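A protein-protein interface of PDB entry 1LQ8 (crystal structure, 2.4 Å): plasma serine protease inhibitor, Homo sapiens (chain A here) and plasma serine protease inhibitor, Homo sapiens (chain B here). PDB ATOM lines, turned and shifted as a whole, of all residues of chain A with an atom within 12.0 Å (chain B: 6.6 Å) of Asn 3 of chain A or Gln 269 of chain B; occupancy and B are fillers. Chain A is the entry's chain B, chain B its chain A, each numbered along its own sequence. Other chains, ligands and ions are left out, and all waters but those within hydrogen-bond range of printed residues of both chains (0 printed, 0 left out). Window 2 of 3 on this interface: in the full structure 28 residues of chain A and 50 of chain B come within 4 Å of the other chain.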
ATOM      1  N   ASN A   3     -25.910  10.158 -20.558  1.00  0.00           N
ATOM      2  CA  ASN A   3     -26.538  11.410 -20.967  1.00  0.00           C
ATOM      3  C   ASN A   3     -25.717  12.577 -20.446  1.00  0.00           C
ATOM      4  O   ASN A   3     -24.707  12.381 -19.768  1.00  0.00           O
ATOM      5  CB  ASN A   3     -27.956  11.510 -20.400  1.00  0.00           C
ATOM      6  CG  ASN A   3     -28.667  10.180 -20.386  1.00  0.00           C
ATOM      7  OD1 ASN A   3     -28.767   9.509 -21.414  1.00  0.00           O
ATOM      8  ND2 ASN A   3     -29.166   9.785 -19.216  1.00  0.00           N
ATOM      9  N   SER A   4     -26.168  13.787 -20.760  1.00  0.00           N
ATOM     10  CA  SER A   4     -25.486  14.995 -20.327  1.00  0.00           C
ATOM     11  C   SER A   4     -26.508  16.106 -20.127  1.00  0.00           C
ATOM     12  O   SER A   4     -26.784  16.877 -21.045  1.00  0.00           O
ATOM     13  CB  SER A   4     -24.452  15.415 -21.376  1.00  0.00           C
ATOM     14  OG  SER A   4     -23.666  16.502 -20.925  1.00  0.00           O
ATOM     15  N   GLN A   5     -27.076  16.175 -18.924  1.00  0.00           N
ATOM     16  CA  GLN A   5     -28.063  17.204 -18.605  1.00  0.00           C
ATOM     17  C   GLN A   5     -27.411  18.584 -18.585  1.00  0.00           C
ATOM     18  O   GLN A   5     -26.266  18.745 -18.163  1.00  0.00           O
ATOM     19  CB  GLN A   5     -28.712  16.942 -17.242  1.00  0.00           C
ATOM     20  CG  GLN A   5     -29.727  18.010 -16.846  1.00  0.00           C
ATOM     21  CD  GLN A   5     -30.295  17.818 -15.442  1.00  0.00           C
ATOM     22  OE1 GLN A   5     -30.948  16.813 -15.150  1.00  0.00           O
ATOM     23  NE2 GLN A   5     -30.047  18.792 -14.567  1.00  0.00           N
ATOM     24  N   ARG A   6     -28.158  19.581 -19.034  1.00  0.00           N
ATOM     25  CA  ARG A   6     -27.663  20.943 -19.079  1.00  0.00           C
ATOM     26  C   ARG A   6     -28.116  21.700 -17.824  1.00  0.00           C
ATOM     27  O   ARG A   6     -29.251  21.542 -17.376  1.00  0.00           O
ATOM     28  CB  ARG A   6     -28.222  21.626 -20.321  1.00  0.00           C
ATOM     29  CG  ARG A   6     -27.321  22.657 -20.943  1.00  0.00           C
ATOM     30  CD  ARG A   6     -26.794  22.167 -22.285  1.00  0.00           C
ATOM     31  NE  ARG A   6     -26.278  23.263 -23.104  1.00  0.00           N
ATOM     32  CZ  ARG A   6     -26.985  24.340 -23.443  1.00  0.00           C
ATOM     33  NH1 ARG A   6     -28.246  24.470 -23.033  1.00  0.00           N
ATOM     34  NH2 ARG A   6     -26.426  25.289 -24.190  1.00  0.00           N
ATOM     35  N   LEU A   7     -27.227  22.496 -17.242  1.00  0.00           N
ATOM     36  CA  LEU A   7     -27.577  23.290 -16.068  1.00  0.00           C
ATOM     37  C   LEU A   7     -26.891  24.653 -16.187  1.00  0.00           C
ATOM     38  O   LEU A   7     -25.681  24.777 -15.980  1.00  0.00           O
ATOM     39  CB  LEU A   7     -27.160  22.587 -14.763  1.00  0.00           C
ATOM     40  CG  LEU A   7     -27.536  23.340 -13.466  1.00  0.00           C
ATOM     41  CD1 LEU A   7     -29.004  23.747 -13.525  1.00  0.00           C
ATOM     42  CD2 LEU A   7     -27.241  22.489 -12.237  1.00  0.00           C
ATOM     43  N   VAL A   8     -27.677  25.667 -16.530  1.00  0.00           N
ATOM     44  CA  VAL A   8     -27.153  27.008 -16.715  1.00  0.00           C
ATOM     45  C   VAL A   8     -27.724  28.036 -15.738  1.00  0.00           C
ATOM     46  O   VAL A   8     -28.910  28.363 -15.765  1.00  0.00           O
ATOM     47  CB  VAL A   8     -27.406  27.484 -18.171  1.00  0.00           C
ATOM     48  CG1 VAL A   8     -28.867  27.274 -18.536  1.00  0.00           C
ATOM     49  CG2 VAL A   8     -27.033  28.947 -18.323  1.00  0.00           C
ATOM     50  N   GLU B 210     -18.228  20.618 -18.374  1.00  0.00           N
ATOM     51  CA  GLU B 210     -19.049  19.417 -18.398  1.00  0.00           C
ATOM     52  C   GLU B 210     -18.267  18.420 -17.564  1.00  0.00           C
ATOM     53  O   GLU B 210     -17.059  18.266 -17.752  1.00  0.00           O
ATOM     54  CB  GLU B 210     -19.186  18.904 -19.836  1.00  0.00           C
ATOM     55  CG  GLU B 210     -20.411  18.041 -20.099  1.00  0.00           C
ATOM     56  CD  GLU B 210     -20.396  17.395 -21.477  1.00  0.00           C
ATOM     57  OE1 GLU B 210     -20.036  18.079 -22.465  1.00  0.00           O
ATOM     58  OE2 GLU B 210     -20.763  16.200 -21.564  1.00  0.00           O
ATOM     59  N   ASP B 211     -18.939  17.758 -16.631  1.00  0.00           N
ATOM     60  CA  ASP B 211     -18.265  16.787 -15.780  1.00  0.00           C
ATOM     61  C   ASP B 211     -19.301  16.130 -14.860  1.00  0.00           C
ATOM     62  O   ASP B 211     -20.512  16.348 -15.012  1.00  0.00           O
ATOM     63  CB  ASP B 211     -17.146  17.499 -14.981  1.00  0.00           C
ATOM     64  CG  ASP B 211     -16.289  16.539 -14.142  1.00  0.00           C
ATOM     65  OD1 ASP B 211     -16.208  15.341 -14.486  1.00  0.00           O
ATOM     66  OD2 ASP B 211     -15.684  16.992 -13.141  1.00  0.00           O
ATOM     67  N   GLN B 212     -18.821  15.313 -13.927  1.00  0.00           N
ATOM     68  CA  GLN B 212     -19.687  14.630 -12.977  1.00  0.00           C
ATOM     69  C   GLN B 212     -19.823  15.538 -11.755  1.00  0.00           C
ATOM     70  O   GLN B 212     -18.825  15.881 -11.131  1.00  0.00           O
ATOM     71  CB  GLN B 212     -19.050  13.298 -12.565  1.00  0.00           C
ATOM     72  CG  GLN B 212     -20.043  12.182 -12.262  1.00  0.00           C
ATOM     73  CD  GLN B 212     -20.605  11.541 -13.522  1.00  0.00           C
ATOM     74  OE1 GLN B 212     -21.637  10.869 -13.483  1.00  0.00           O
ATOM     75  NE2 GLN B 212     -19.917  11.737 -14.644  1.00  0.00           N
ATOM     76  N   TYR B 213     -21.049  15.931 -11.421  1.00  0.00           N
ATOM     77  CA  TYR B 213     -21.309  16.803 -10.265  1.00  0.00           C
ATOM     78  C   TYR B 213     -22.357  16.174  -9.354  1.00  0.00           C
ATOM     79  O   TYR B 213     -23.149  15.346  -9.799  1.00  0.00           O
ATOM     80  CB  TYR B 213     -21.877  18.156 -10.709  1.00  0.00           C
ATOM     81  CG  TYR B 213     -20.989  19.000 -11.579  1.00  0.00           C
ATOM     82  CD1 TYR B 213     -19.913  19.699 -11.037  1.00  0.00           C
ATOM     83  CD2 TYR B 213     -21.230  19.110 -12.945  1.00  0.00           C
ATOM     84  CE1 TYR B 213     -19.086  20.497 -11.835  1.00  0.00           C
ATOM     85  CE2 TYR B 213     -20.409  19.904 -13.763  1.00  0.00           C
ATOM     86  CZ  TYR B 213     -19.335  20.594 -13.202  1.00  0.00           C
ATOM     87  OH  TYR B 213     -18.508  21.355 -14.009  1.00  0.00           O
ATOM     88  N   LYS B 267     -24.349  11.836  -7.919  1.00  0.00           N
ATOM     89  CA  LYS B 267     -23.574  12.383  -9.034  1.00  0.00           C
ATOM     90  C   LYS B 267     -24.230  12.177 -10.381  1.00  0.00           C
ATOM     91  O   LYS B 267     -24.861  11.152 -10.631  1.00  0.00           O
ATOM     92  CB  LYS B 267     -22.162  11.794  -9.059  1.00  0.00           C
ATOM     93  CG  LYS B 267     -21.267  12.356  -7.976  1.00  0.00           C
ATOM     94  CD  LYS B 267     -19.811  12.151  -8.311  1.00  0.00           C
ATOM     95  CE  LYS B 267     -18.917  12.849  -7.302  1.00  0.00           C
ATOM     96  NZ  LYS B 267     -17.469  12.639  -7.613  1.00  0.00           N
ATOM     97  N   ARG B 268     -24.076  13.162 -11.255  1.00  0.00           N
ATOM     98  CA  ARG B 268     -24.666  13.085 -12.577  1.00  0.00           C
ATOM     99  C   ARG B 268     -23.821  13.803 -13.625  1.00  0.00           C
ATOM    100  O   ARG B 268     -23.135  14.777 -13.328  1.00  0.00           O
ATOM    101  CB  ARG B 268     -26.078  13.679 -12.564  1.00  0.00           C
ATOM    102  CG  ARG B 268     -26.838  13.398 -13.843  1.00  0.00           C
ATOM    103  CD  ARG B 268     -27.838  14.488 -14.166  1.00  0.00           C
ATOM    104  NE  ARG B 268     -29.046  14.434 -13.345  1.00  0.00           N
ATOM    105  CZ  ARG B 268     -29.947  13.456 -13.395  1.00  0.00           C
ATOM    106  NH1 ARG B 268     -29.780  12.429 -14.227  1.00  0.00           N
ATOM    107  NH2 ARG B 268     -31.030  13.519 -12.627  1.00  0.00           N
ATOM    108  N   GLN B 269     -23.864  13.295 -14.852  1.00  0.00           N
ATOM    109  CA  GLN B 269     -23.139  13.893 -15.959  1.00  0.00           C
ATOM    110  C   GLN B 269     -23.853  15.218 -16.243  1.00  0.00           C
ATOM    111  O   GLN B 269     -25.029  15.245 -16.623  1.00  0.00           O
ATOM    112  CB  GLN B 269     -23.196  12.964 -17.170  1.00  0.00           C
ATOM    113  CG  GLN B 269     -22.567  13.525 -18.422  1.00  0.00           C
ATOM    114  CD  GLN B 269     -21.171  14.030 -18.192  1.00  0.00           C
ATOM    115  OE1 GLN B 269     -20.387  13.420 -17.460  1.00  0.00           O
ATOM    116  NE2 GLN B 269     -20.839  15.146 -18.827  1.00  0.00           N
ATOM    117  N   LEU B 270     -23.130  16.316 -16.049  1.00  0.00           N
ATOM    118  CA  LEU B 270     -23.699  17.650 -16.223  1.00  0.00           C
ATOM    119  C   LEU B 270     -22.819  18.602 -17.029  1.00  0.00           C
ATOM    120  O   LEU B 270     -21.583  18.580 -16.931  1.00  0.00           O
ATOM    121  CB  LEU B 270     -23.938  18.271 -14.841  1.00  0.00           C
ATOM    122  CG  LEU B 270     -25.311  18.761 -14.377  1.00  0.00           C
ATOM    123  CD1 LEU B 270     -26.298  17.599 -14.317  1.00  0.00           C
ATOM    124  CD2 LEU B 270     -25.163  19.397 -13.000  1.00  0.00           C
ATOM    125  N   GLU B 271     -23.460  19.431 -17.838  1.00  0.00           N
ATOM    126  CA  GLU B 271     -22.727  20.429 -18.584  1.00  0.00           C
ATOM    127  C   GLU B 271     -23.116  21.734 -17.874  1.00  0.00           C
ATOM    128  O   GLU B 271     -24.062  22.429 -18.255  1.00  0.00           O
ATOM    129  CB  GLU B 271     -23.143  20.444 -20.049  1.00  0.00           C
ATOM    130  CG  GLU B 271     -22.083  21.095 -20.930  1.00  0.00           C
ATOM    131  CD  GLU B 271     -22.478  21.168 -22.389  1.00  0.00           C
ATOM    132  OE1 GLU B 271     -21.601  21.513 -23.215  1.00  0.00           O
ATOM    133  OE2 GLU B 271     -23.659  20.890 -22.703  1.00  0.00           O
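The backbone carbonyl oxygen of Gln 269 of chain B sits at hydrogen-bond distance from the backbone NH of Gln 5 of chain A (3.2 Å). The side-chain carboxylate (OE2) of Glu 271 of chain B lies within salt-bridge range of the guanidinium group (NE) of Arg 6 of chain A. The side-chain carboxylate of Glu 210 of chain B sits at hydrogen-bond distance from the side-chain hydroxyl of Ser 4 of chain A, at 3.0 Å. The backbone carbonyl oxygen (O) of Glu 271 of chain B lies within hydrogen-bond range of the backbone NH (N) of Leu 7 of chain A, at 3.3 Å. N of Glu 271 of chain B sits at hydrogen-bond distance from O of Gln 5 of chain A, 2.9 Å away.
The side-chain carboxylate (OE2) of Glu 210 of chain B sits at hydrogen-bond distance from the side-chain amide nitrogen (NE2) of Gln 269 of chain B (2.9 Å). The side-chain amide nitrogen (NE2) of Gln 212 of chain B lies within hydrogen-bond range of the side-chain amide oxygen (OE1) of Gln 269 of chain B. The backbone NH of Asp 211 of chain B sits at hydrogen-bond distance from the backbone carbonyl oxygen of Leu 270 of chain B (2.8 Å). N of Arg 268 of chain B lies within hydrogen-bond range of O of Tyr 213 of chain B.
Among the printed residues, pairs that only touch across the chains: Asn 3 of chain A with Gln 269 of chain B (2.8 Å), Ser 4 of chain A with Gln 269 of chain B (3.7 Å), Gln 5 of chain A with Arg 268 of chain B (3.5 Å), Gln 5 of chain A with Leu 270 of chain B (3.4 Å) and Leu 7 of chain A with Leu 270 of chain B (3.8 Å).
Asn 3 of chain A touches just one residue of chain B: Gln 269. Of the printed residues of chain B, Ser 4 of chain A touches Glu 210 and Gln 269. Printed residues of chain B within 4 Å of Arg 6 of chain A: Glu 271 (3.4 Å). Of the printed residues of chain B, Leu 7 of chain A touches Leu 270 and Glu 271. Val 8 of chain A touches none of the printed residues of chain B. Of chain A, only Ser 4 comes within 4 Å of Glu 210 of chain B. No residue of chain A comes within 4 Å of Gln 212 of chain B. Lys 267 of chain B touches none of the printed residues of chain A. Arg 268 of chain B touches one residue of chain A. Leu 270 of chain B touches two residues of chain A. Of chain A, only Gln 5 (2.9 Å), Arg 6 (3.4 Å) and Leu 7 (3.3 Å) come within 4 Å of Glu 271 of chain B. The nearest residue of chain B that does not touch Asn 3 of chain A is Leu 270 of chain B (5.6 Å). The nearest printed residue of chain B that does not touch Leu 7 of chain A is Tyr 213 of chain B (6.9 Å).
Printed residues of chain B that touch a printed residue of chain A: Glu 210, Arg 268, Gln 269, Leu 270 and Glu 271. Hydrophobic or aromatic side chains of chain B within 4 Å of the printed part of chain A: Leu 270. Among the printed residues, Asp or Glu carboxylates within 4 Å of a Lys or Arg side-chain nitrogen of the other chain: Arg 6 of chain A with Glu 271 of chain B (3.6 Å).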
